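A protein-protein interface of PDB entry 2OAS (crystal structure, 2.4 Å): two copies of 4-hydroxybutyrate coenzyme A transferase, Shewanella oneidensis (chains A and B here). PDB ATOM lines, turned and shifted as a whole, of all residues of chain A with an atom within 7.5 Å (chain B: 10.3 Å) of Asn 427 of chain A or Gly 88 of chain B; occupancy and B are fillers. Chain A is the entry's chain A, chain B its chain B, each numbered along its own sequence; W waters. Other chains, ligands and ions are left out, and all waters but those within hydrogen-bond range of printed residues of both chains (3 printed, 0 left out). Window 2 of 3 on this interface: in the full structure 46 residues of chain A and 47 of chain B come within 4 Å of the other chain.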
ATOM      1  N   ARG A 398      18.132 -13.638 -19.893  1.00  0.00           N
ATOM      2  CA  ARG A 398      17.636 -12.269 -19.893  1.00  0.00           C
ATOM      3  C   ARG A 398      17.365 -11.781 -21.321  1.00  0.00           C
ATOM      4  O   ARG A 398      16.440 -11.003 -21.559  1.00  0.00           O
ATOM      5  CB  ARG A 398      18.601 -11.328 -19.180  1.00  0.00           C
ATOM      6  CG  ARG A 398      19.936 -11.140 -19.868  1.00  0.00           C
ATOM      7  CD  ARG A 398      20.754 -10.067 -19.152  1.00  0.00           C
ATOM      8  NE  ARG A 398      22.043  -9.832 -19.794  1.00  0.00           N
ATOM      9  CZ  ARG A 398      22.950  -8.963 -19.356  1.00  0.00           C
ATOM     10  NH1 ARG A 398      22.706  -8.244 -18.268  1.00  0.00           N
ATOM     11  NH2 ARG A 398      24.100  -8.808 -20.011  1.00  0.00           N
ATOM     12  N   GLU A 399      18.166 -12.248 -22.271  1.00  0.00           N
ATOM     13  CA  GLU A 399      17.989 -11.859 -23.668  1.00  0.00           C
ATOM     14  C   GLU A 399      16.698 -12.455 -24.219  1.00  0.00           C
ATOM     15  O   GLU A 399      15.957 -11.790 -24.948  1.00  0.00           O
ATOM     16  CB  GLU A 399      19.180 -12.326 -24.504  1.00  0.00           C
ATOM     17  CG  GLU A 399      20.476 -11.593 -24.170  1.00  0.00           C
ATOM     18  CD  GLU A 399      21.688 -12.088 -24.956  1.00  0.00           C
ATOM     19  OE1 GLU A 399      22.735 -11.405 -24.902  1.00  0.00           O
ATOM     20  OE2 GLU A 399      21.596 -13.149 -25.616  1.00  0.00           O
ATOM     21  N   GLN A 402      13.654 -10.764 -22.601  1.00  0.00           N
ATOM     22  CA  GLN A 402      13.475  -9.448 -23.190  1.00  0.00           C
ATOM     23  C   GLN A 402      12.783  -9.558 -24.549  1.00  0.00           C
ATOM     24  O   GLN A 402      11.765  -8.905 -24.784  1.00  0.00           O
ATOM     25  CB  GLN A 402      14.826  -8.743 -23.331  1.00  0.00           C
ATOM     26  CG  GLN A 402      14.737  -7.370 -23.950  1.00  0.00           C
ATOM     27  CD  GLN A 402      13.845  -6.426 -23.150  1.00  0.00           C
ATOM     28  OE1 GLN A 402      14.211  -5.960 -22.065  1.00  0.00           O
ATOM     29  NE2 GLN A 402      12.659  -6.144 -23.685  1.00  0.00           N
ATOM     30  N   ALA A 420      10.004 -10.921 -14.598  1.00  0.00           N
ATOM     31  CA  ALA A 420      11.293 -11.212 -15.224  1.00  0.00           C
ATOM     32  C   ALA A 420      12.388 -11.071 -14.182  1.00  0.00           C
ATOM     33  O   ALA A 420      13.425 -11.732 -14.242  1.00  0.00           O
ATOM     34  CB  ALA A 420      11.554 -10.248 -16.368  1.00  0.00           C
ATOM     35  N   PHE A 421      12.152 -10.185 -13.227  1.00  0.00           N
ATOM     36  CA  PHE A 421      13.106  -9.952 -12.169  1.00  0.00           C
ATOM     37  C   PHE A 421      12.656 -10.588 -10.862  1.00  0.00           C
ATOM     38  O   PHE A 421      13.466 -11.116 -10.116  1.00  0.00           O
ATOM     39  CB  PHE A 421      13.297  -8.457 -11.958  1.00  0.00           C
ATOM     40  CG  PHE A 421      14.046  -8.119 -10.709  1.00  0.00           C
ATOM     41  CD1 PHE A 421      15.417  -8.303 -10.635  1.00  0.00           C
ATOM     42  CD2 PHE A 421      13.371  -7.651  -9.589  1.00  0.00           C
ATOM     43  CE1 PHE A 421      16.106  -8.031  -9.461  1.00  0.00           C
ATOM     44  CE2 PHE A 421      14.049  -7.378  -8.415  1.00  0.00           C
ATOM     45  CZ  PHE A 421      15.419  -7.566  -8.351  1.00  0.00           C
ATOM     46  N   TRP A 424      12.384 -14.774 -12.071  1.00  0.00           N
ATOM     47  CA  TRP A 424      13.604 -15.353 -12.624  1.00  0.00           C
ATOM     48  C   TRP A 424      14.863 -14.679 -12.095  1.00  0.00           C
ATOM     49  O   TRP A 424      15.960 -15.199 -12.249  1.00  0.00           O
ATOM     50  CB  TRP A 424      13.590 -15.287 -14.160  1.00  0.00           C
ATOM     51  CG  TRP A 424      12.486 -16.091 -14.791  1.00  0.00           C
ATOM     52  CD1 TRP A 424      11.217 -15.672 -15.067  1.00  0.00           C
ATOM     53  CD2 TRP A 424      12.537 -17.476 -15.160  1.00  0.00           C
ATOM     54  NE1 TRP A 424      10.476 -16.707 -15.585  1.00  0.00           N
ATOM     55  CE2 TRP A 424      11.263 -17.821 -15.659  1.00  0.00           C
ATOM     56  CE3 TRP A 424      13.544 -18.454 -15.135  1.00  0.00           C
ATOM     57  CZ2 TRP A 424      10.957 -19.118 -16.107  1.00  0.00           C
ATOM     58  CZ3 TRP A 424      13.241 -19.739 -15.579  1.00  0.00           C
ATOM     59  CH2 TRP A 424      11.961 -20.056 -16.068  1.00  0.00           C
ATOM     60  N   GLY A 425      14.706 -13.521 -11.466  1.00  0.00           N
ATOM     61  CA  GLY A 425      15.858 -12.816 -10.939  1.00  0.00           C
ATOM     62  C   GLY A 425      16.729 -12.280 -12.053  1.00  0.00           C
ATOM     63  O   GLY A 425      17.958 -12.230 -11.941  1.00  0.00           O
ATOM     64  N   LEU A 426      16.099 -11.887 -13.145  1.00  0.00           N
ATOM     65  CA  LEU A 426      16.853 -11.353 -14.257  1.00  0.00           C
ATOM     66  C   LEU A 426      16.659  -9.859 -14.310  1.00  0.00           C
ATOM     67  O   LEU A 426      15.576  -9.360 -14.023  1.00  0.00           O
ATOM     68  CB  LEU A 426      16.367 -11.957 -15.567  1.00  0.00           C
ATOM     69  CG  LEU A 426      16.336 -13.477 -15.653  1.00  0.00           C
ATOM     70  CD1 LEU A 426      15.641 -13.861 -16.946  1.00  0.00           C
ATOM     71  CD2 LEU A 426      17.745 -14.047 -15.593  1.00  0.00           C
ATOM     72  N   ASN A 427      17.712  -9.135 -14.665  1.00  0.00           N
ATOM     73  CA  ASN A 427      17.579  -7.696 -14.784  1.00  0.00           C
ATOM     74  C   ASN A 427      17.904  -7.301 -16.218  1.00  0.00           C
ATOM     75  O   ASN A 427      19.040  -7.411 -16.682  1.00  0.00           O
ATOM     76  CB  ASN A 427      18.463  -6.968 -13.757  1.00  0.00           C
ATOM     77  CG  ASN A 427      19.908  -7.351 -13.855  1.00  0.00           C
ATOM     78  OD1 ASN A 427      20.591  -7.013 -14.822  1.00  0.00           O
ATOM     79  ND2 ASN A 427      20.398  -8.055 -12.842  1.00  0.00           N
ATOM     80  N   LEU A 428      16.853  -6.873 -16.912  1.00  0.00           N
ATOM     81  CA  LEU A 428      16.890  -6.440 -18.309  1.00  0.00           C
ATOM     82  C   LEU A 428      17.384  -4.994 -18.420  1.00  0.00           C
ATOM     83  O   LEU A 428      17.626  -4.370 -17.355  1.00  0.00           O
ATOM     84  CB  LEU A 428      15.473  -6.553 -18.892  1.00  0.00           C
ATOM     85  CG  LEU A 428      14.620  -7.734 -18.405  1.00  0.00           C
ATOM     86  CD1 LEU A 428      13.256  -7.694 -19.091  1.00  0.00           C
ATOM     87  CD2 LEU A 428      15.328  -9.063 -18.697  1.00  0.00           C
ATOM     88  N   LEU B  67      33.684  -7.495 -11.741  1.00  0.00           N
ATOM     89  CA  LEU B  67      32.375  -7.000 -12.158  1.00  0.00           C
ATOM     90  C   LEU B  67      32.535  -5.671 -12.877  1.00  0.00           C
ATOM     91  O   LEU B  67      33.090  -4.709 -12.333  1.00  0.00           O
ATOM     92  CB  LEU B  67      31.446  -6.835 -10.954  1.00  0.00           C
ATOM     93  CG  LEU B  67      31.097  -8.120 -10.186  1.00  0.00           C
ATOM     94  CD1 LEU B  67      30.246  -7.770  -8.973  1.00  0.00           C
ATOM     95  CD2 LEU B  67      30.359  -9.101 -11.095  1.00  0.00           C
ATOM     96  N   GLY B  68      32.053  -5.627 -14.112  1.00  0.00           N
ATOM     97  CA  GLY B  68      32.167  -4.410 -14.887  1.00  0.00           C
ATOM     98  C   GLY B  68      33.276  -4.534 -15.908  1.00  0.00           C
ATOM     99  O   GLY B  68      33.328  -3.771 -16.876  1.00  0.00           O
ATOM    100  N   LEU B  70      34.573  -8.001 -16.783  1.00  0.00           N
ATOM    101  CA  LEU B  70      34.312  -9.267 -17.445  1.00  0.00           C
ATOM    102  C   LEU B  70      33.001  -9.879 -16.985  1.00  0.00           C
ATOM    103  O   LEU B  70      32.607  -9.721 -15.834  1.00  0.00           O
ATOM    104  CB  LEU B  70      35.470 -10.224 -17.151  1.00  0.00           C
ATOM    105  CG  LEU B  70      35.279 -11.707 -17.437  1.00  0.00           C
ATOM    106  CD1 LEU B  70      34.671 -11.907 -18.799  1.00  0.00           C
ATOM    107  CD2 LEU B  70      36.617 -12.397 -17.357  1.00  0.00           C
ATOM    108  N   ARG B  71      32.318 -10.574 -17.882  1.00  0.00           N
ATOM    109  CA  ARG B  71      31.055 -11.217 -17.538  1.00  0.00           C
ATOM    110  C   ARG B  71      31.055 -12.627 -18.108  1.00  0.00           C
ATOM    111  O   ARG B  71      31.483 -12.840 -19.233  1.00  0.00           O
ATOM    112  CB  ARG B  71      29.871 -10.411 -18.100  1.00  0.00           C
ATOM    113  CG  ARG B  71      28.504 -11.118 -18.015  1.00  0.00           C
ATOM    114  CD  ARG B  71      27.325 -10.216 -18.437  1.00  0.00           C
ATOM    115  NE  ARG B  71      26.711  -9.551 -17.284  1.00  0.00           N
ATOM    116  CZ  ARG B  71      25.566  -9.926 -16.709  1.00  0.00           C
ATOM    117  NH1 ARG B  71      24.886 -10.959 -17.180  1.00  0.00           N
ATOM    118  NH2 ARG B  71      25.114  -9.280 -15.640  1.00  0.00           N
ATOM    119  N   HIS B  72      30.589 -13.594 -17.320  1.00  0.00           N
ATOM    120  CA  HIS B  72      30.539 -14.982 -17.758  1.00  0.00           C
ATOM    121  C   HIS B  72      29.271 -15.293 -18.556  1.00  0.00           C
ATOM    122  O   HIS B  72      28.174 -14.874 -18.170  1.00  0.00           O
ATOM    123  CB  HIS B  72      30.621 -15.915 -16.540  1.00  0.00           C
ATOM    124  CG  HIS B  72      31.887 -15.769 -15.755  1.00  0.00           C
ATOM    125  ND1 HIS B  72      32.020 -14.878 -14.707  1.00  0.00           N
ATOM    126  CD2 HIS B  72      33.107 -16.344 -15.916  1.00  0.00           C
ATOM    127  CE1 HIS B  72      33.263 -14.910 -14.258  1.00  0.00           C
ATOM    128  NE2 HIS B  72      33.944 -15.791 -14.975  1.00  0.00           N
ATOM    129  N   THR B  81      30.276 -20.321 -10.941  1.00  0.00           N
ATOM    130  CA  THR B  81      29.347 -19.478 -11.674  1.00  0.00           C
ATOM    131  C   THR B  81      27.924 -19.475 -11.126  1.00  0.00           C
ATOM    132  O   THR B  81      27.199 -18.499 -11.319  1.00  0.00           O
ATOM    133  CB  THR B  81      29.313 -19.881 -13.152  1.00  0.00           C
ATOM    134  OG1 THR B  81      29.141 -21.299 -13.250  1.00  0.00           O
ATOM    135  CG2 THR B  81      30.605 -19.478 -13.849  1.00  0.00           C
ATOM    136  N   ARG B  82      27.527 -20.545 -10.442  1.00  0.00           N
ATOM    137  CA  ARG B  82      26.174 -20.634  -9.878  1.00  0.00           C
ATOM    138  C   ARG B  82      25.755 -19.400  -9.077  1.00  0.00           C
ATOM    139  O   ARG B  82      24.681 -18.844  -9.304  1.00  0.00           O
ATOM    140  CB  ARG B  82      26.038 -21.869  -8.977  1.00  0.00           C
ATOM    141  CG  ARG B  82      25.976 -23.181  -9.723  1.00  0.00           C
ATOM    142  CD  ARG B  82      26.162 -24.375  -8.799  1.00  0.00           C
ATOM    143  NE  ARG B  82      26.700 -25.503  -9.555  1.00  0.00           N
ATOM    144  CZ  ARG B  82      27.455 -26.468  -9.041  1.00  0.00           C
ATOM    145  NH1 ARG B  82      27.768 -26.457  -7.754  1.00  0.00           N
ATOM    146  NH2 ARG B  82      27.921 -27.430  -9.830  1.00  0.00           N
ATOM    147  N   PRO B  83      26.594 -18.965  -8.123  1.00  0.00           N
ATOM    148  CA  PRO B  83      26.232 -17.795  -7.332  1.00  0.00           C
ATOM    149  C   PRO B  83      26.053 -16.562  -8.201  1.00  0.00           C
ATOM    150  O   PRO B  83      25.231 -15.696  -7.903  1.00  0.00           O
ATOM    151  CB  PRO B  83      27.407 -17.663  -6.366  1.00  0.00           C
ATOM    152  CG  PRO B  83      28.549 -18.175  -7.182  1.00  0.00           C
ATOM    153  CD  PRO B  83      27.961 -19.411  -7.790  1.00  0.00           C
ATOM    154  N   LEU B  84      26.832 -16.485  -9.273  1.00  0.00           N
ATOM    155  CA  LEU B  84      26.746 -15.348 -10.174  1.00  0.00           C
ATOM    156  C   LEU B  84      25.504 -15.435 -11.049  1.00  0.00           C
ATOM    157  O   LEU B  84      24.866 -14.424 -11.329  1.00  0.00           O
ATOM    158  CB  LEU B  84      28.004 -15.253 -11.042  1.00  0.00           C
ATOM    159  CG  LEU B  84      29.141 -14.339 -10.562  1.00  0.00           C
ATOM    160  CD1 LEU B  84      29.538 -14.672  -9.138  1.00  0.00           C
ATOM    161  CD2 LEU B  84      30.331 -14.491 -11.514  1.00  0.00           C
ATOM    162  N   LEU B  85      25.153 -16.639 -11.479  1.00  0.00           N
ATOM    163  CA  LEU B  85      23.962 -16.808 -12.313  1.00  0.00           C
ATOM    164  C   LEU B  85      22.705 -16.491 -11.499  1.00  0.00           C
ATOM    165  O   LEU B  85      21.828 -15.745 -11.950  1.00  0.00           O
ATOM    166  CB  LEU B  85      23.896 -18.231 -12.865  1.00  0.00           C
ATOM    167  CG  LEU B  85      24.953 -18.549 -13.926  1.00  0.00           C
ATOM    168  CD1 LEU B  85      25.041 -20.045 -14.165  1.00  0.00           C
ATOM    169  CD2 LEU B  85      24.602 -17.812 -15.208  1.00  0.00           C
ATOM    170  N   GLN B  86      22.646 -17.055 -10.294  1.00  0.00           N
ATOM    171  CA  GLN B  86      21.525 -16.857  -9.386  1.00  0.00           C
ATOM    172  C   GLN B  86      21.422 -15.396  -8.968  1.00  0.00           C
ATOM    173  O   GLN B  86      20.332 -14.897  -8.690  1.00  0.00           O
ATOM    174  CB  GLN B  86      21.676 -17.753  -8.146  1.00  0.00           C
ATOM    175  CG  GLN B  86      21.725 -19.260  -8.476  1.00  0.00           C
ATOM    176  CD  GLN B  86      21.824 -20.167  -7.240  1.00  0.00           C
ATOM    177  OE1 GLN B  86      22.667 -19.963  -6.365  1.00  0.00           O
ATOM    178  NE2 GLN B  86      20.963 -21.183  -7.179  1.00  0.00           N
ATOM    179  N   SER B  87      22.557 -14.709  -8.935  1.00  0.00           N
ATOM    180  CA  SER B  87      22.571 -13.303  -8.543  1.00  0.00           C
ATOM    181  C   SER B  87      22.420 -12.400  -9.756  1.00  0.00           C
ATOM    182  O   SER B  87      22.517 -11.176  -9.646  1.00  0.00           O
ATOM    183  CB  SER B  87      23.871 -12.972  -7.810  1.00  0.00           C
ATOM    184  OG  SER B  87      24.988 -13.215  -8.642  1.00  0.00           O
ATOM    185  N   GLY B  88      22.189 -13.019 -10.913  1.00  0.00           N
ATOM    186  CA  GLY B  88      22.019 -12.274 -12.148  1.00  0.00           C
ATOM    187  C   GLY B  88      23.247 -11.509 -12.620  1.00  0.00           C
ATOM    188  O   GLY B  88      23.113 -10.530 -13.353  1.00  0.00           O
ATOM    189  N   ASP B  89      24.440 -11.941 -12.213  1.00  0.00           N
ATOM    190  CA  ASP B  89      25.673 -11.271 -12.613  1.00  0.00           C
ATOM    191  C   ASP B  89      26.286 -11.956 -13.815  1.00  0.00           C
ATOM    192  O   ASP B  89      27.189 -11.422 -14.453  1.00  0.00           O
ATOM    193  CB  ASP B  89      26.695 -11.279 -11.485  1.00  0.00           C
ATOM    194  CG  ASP B  89      26.214 -10.530 -10.264  1.00  0.00           C
ATOM    195  OD1 ASP B  89      25.819  -9.348 -10.406  1.00  0.00           O
ATOM    196  OD2 ASP B  89      26.233 -11.119  -9.165  1.00  0.00           O
ATOM    197  N   ALA B  90      25.796 -13.151 -14.108  1.00  0.00           N
ATOM    198  CA  ALA B  90      26.285 -13.911 -15.241  1.00  0.00           C
ATOM    199  C   ALA B  90      25.095 -14.315 -16.101  1.00  0.00           C
ATOM    200  O   ALA B  90      23.944 -14.219 -15.665  1.00  0.00           O
ATOM    201  CB  ALA B  90      27.035 -15.150 -14.758  1.00  0.00           C
ATOM    202  N   ASP B  91      25.379 -14.767 -17.316  1.00  0.00           N
ATOM    203  CA  ASP B  91      24.328 -15.166 -18.239  1.00  0.00           C
ATOM    204  C   ASP B  91      24.354 -16.645 -18.536  1.00  0.00           C
ATOM    205  O   ASP B  91      25.419 -17.212 -18.729  1.00  0.00           O
ATOM    206  CB  ASP B  91      24.466 -14.400 -19.549  1.00  0.00           C
ATOM    207  CG  ASP B  91      24.258 -12.921 -19.369  1.00  0.00           C
ATOM    208  OD1 ASP B  91      23.281 -12.558 -18.676  1.00  0.00           O
ATOM    209  OD2 ASP B  91      25.052 -12.126 -19.910  1.00  0.00           O
ATOM    210  N   TYR B  92      23.178 -17.263 -18.568  1.00  0.00           N
ATOM    211  CA  TYR B  92      23.050 -18.681 -18.873  1.00  0.00           C
ATOM    212  C   TYR B  92      22.341 -18.859 -20.209  1.00  0.00           C
ATOM    213  O   TYR B  92      21.211 -18.405 -20.387  1.00  0.00           O
ATOM    214  CB  TYR B  92      22.261 -19.405 -17.796  1.00  0.00           C
ATOM    215  CG  TYR B  92      21.830 -20.808 -18.184  1.00  0.00           C
ATOM    216  CD1 TYR B  92      20.481 -21.149 -18.261  1.00  0.00           C
ATOM    217  CD2 TYR B  92      22.773 -21.805 -18.448  1.00  0.00           C
ATOM    218  CE1 TYR B  92      20.083 -22.443 -18.583  1.00  0.00           C
ATOM    219  CE2 TYR B  92      22.381 -23.103 -18.773  1.00  0.00           C
ATOM    220  CZ  TYR B  92      21.036 -23.411 -18.833  1.00  0.00           C
ATOM    221  OH  TYR B  92      20.652 -24.700 -19.107  1.00  0.00           O
ATOM    222  N   THR B 323      13.920 -21.526 -10.762  1.00  0.00           N
ATOM    223  CA  THR B 323      14.394 -20.526 -11.705  1.00  0.00           C
ATOM    224  C   THR B 323      15.891 -20.285 -11.554  1.00  0.00           C
ATOM    225  O   THR B 323      16.491 -19.536 -12.330  1.00  0.00           O
ATOM    226  CB  THR B 323      13.683 -19.196 -11.503  1.00  0.00           C
ATOM    227  OG1 THR B 323      13.999 -18.693 -10.207  1.00  0.00           O
ATOM    228  CG2 THR B 323      12.172 -19.380 -11.616  1.00  0.00           C
ATOM    229  N   LYS B 324      16.495 -20.915 -10.550  1.00  0.00           N
ATOM    230  CA  LYS B 324      17.925 -20.765 -10.327  1.00  0.00           C
ATOM    231  C   LYS B 324      18.683 -21.839 -11.086  1.00  0.00           C
ATOM    232  O   LYS B 324      18.520 -23.031 -10.821  1.00  0.00           O
ATOM    233  CB  LYS B 324      18.255 -20.857  -8.837  1.00  0.00           C
ATOM    234  CG  LYS B 324      17.148 -21.450  -7.994  1.00  0.00           C
ATOM    235  CD  LYS B 324      16.321 -20.348  -7.299  1.00  0.00           C
ATOM    236  CE  LYS B 324      14.867 -20.280  -7.799  1.00  0.00           C
ATOM    237  NZ  LYS B 324      14.067 -21.528  -7.577  1.00  0.00           N
ATOM    238  N   ILE B 325      19.509 -21.407 -12.034  1.00  0.00           N
ATOM    239  CA  ILE B 325      20.294 -22.325 -12.856  1.00  0.00           C
ATOM    240  C   ILE B 325      21.396 -22.988 -12.056  1.00  0.00           C
ATOM    241  O   ILE B 325      22.204 -22.318 -11.418  1.00  0.00           O
ATOM    242  CB  ILE B 325      20.934 -21.593 -14.037  1.00  0.00           C
ATOM    243  CG1 ILE B 325      19.884 -20.757 -14.769  1.00  0.00           C
ATOM    244  CG2 ILE B 325      21.566 -22.613 -14.994  1.00  0.00           C
ATOM    245  CD1 ILE B 325      18.687 -21.544 -15.249  1.00  0.00           C
HETATM  246  O   HOH W   1      17.068 -17.137 -13.815  1.00  0.00           O
HETATM  247  O   HOH W   2      22.901 -11.535 -21.749  1.00  0.00           O
HETATM  248  O   HOH W   3      20.755 -14.786 -18.233  1.00  0.00           O
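Water W1 bridges O of Trp 424 of chain A and O of Thr 323 of chain B.
Water W2 lies within hydrogen-bond range of NE of Arg 398 of chain A, OD2 of Asp 91 of chain B and OE1 of Glu 399 of chain A.
Water W3 lies within hydrogen-bond range of N of Arg 398 of chain A (3.3 Å), OD1 of Asp 91 of chain B (3.4 Å) and N of Tyr 92 of chain B (3.5 Å).
NH2 of Arg 71 of chain B sits at hydrogen-bond distance from O of Gly 88 of chain B.
The backbone carbonyl oxygen of Asp 89 of chain B lies close to the guanidinium group of Arg 71 of chain B, 3.2 Å away.
The guanidinium group (NH1) of Arg 71 of chain B is in salt-bridge range of the side-chain carboxylate (OD1) of Asp 91 of chain B.
O of His 72 of chain B sits at hydrogen-bond distance from N of Asp 91 of chain B, at 2.9 Å.
Among the printed residues, pairs that only touch across the chains: Arg 398 of chain A with Arg 71 of chain B (3.5 Å), Asn 427 of chain A with Gly 88 of chain B (3.7 Å) and Trp 424 of chain A with Thr 323 of chain B (3.7 Å).
No position is printed for both chains.
Of the 4 pairs that touch across the chains among the printed residues, none has its exchanged pair printed and touching as well.
NE of Arg 398 of chain A lies within salt-bridge range of OD1 of Asp 91 of chain B (3.2 Å).
Printed residues of chain A that touch a printed residue of chain B: Arg 398, Trp 424 and Asn 427.
Hydrophobic or aromatic side chains of chain A within 4 Å of the printed part of chain B: Trp 424.
Of the printed residues of chain B, Arg 398 of chain A touches Arg 71 (3.5 Å) and Asp 91 (3.2 Å).
Phe 421 of chain A touches none of the printed residues of chain B.
Printed residues of chain B within 4 Å of Trp 424 of chain A: Thr 323.
No residue of chain B comes within 4 Å of Leu 426 of chain A.
Asn 427 of chain A touches just one residue of chain B: Gly 88 (3.7 Å).
No residue of chain B comes within 4 Å of Leu 428 of chain A.
Of the printed residues of chain A, Arg 71 of chain B touches Arg 398 (3.5 Å).
Printed residues of chain A within 4 Å of Gly 88 of chain B: Asn 427 (3.7 Å).
Of the printed residues of chain A, Asp 91 of chain B touches Arg 398 (3.2 Å).
The nearest printed residue of chain B that does not touch Trp 424 of chain A is Gln 86 of chain B (5.6 Å).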
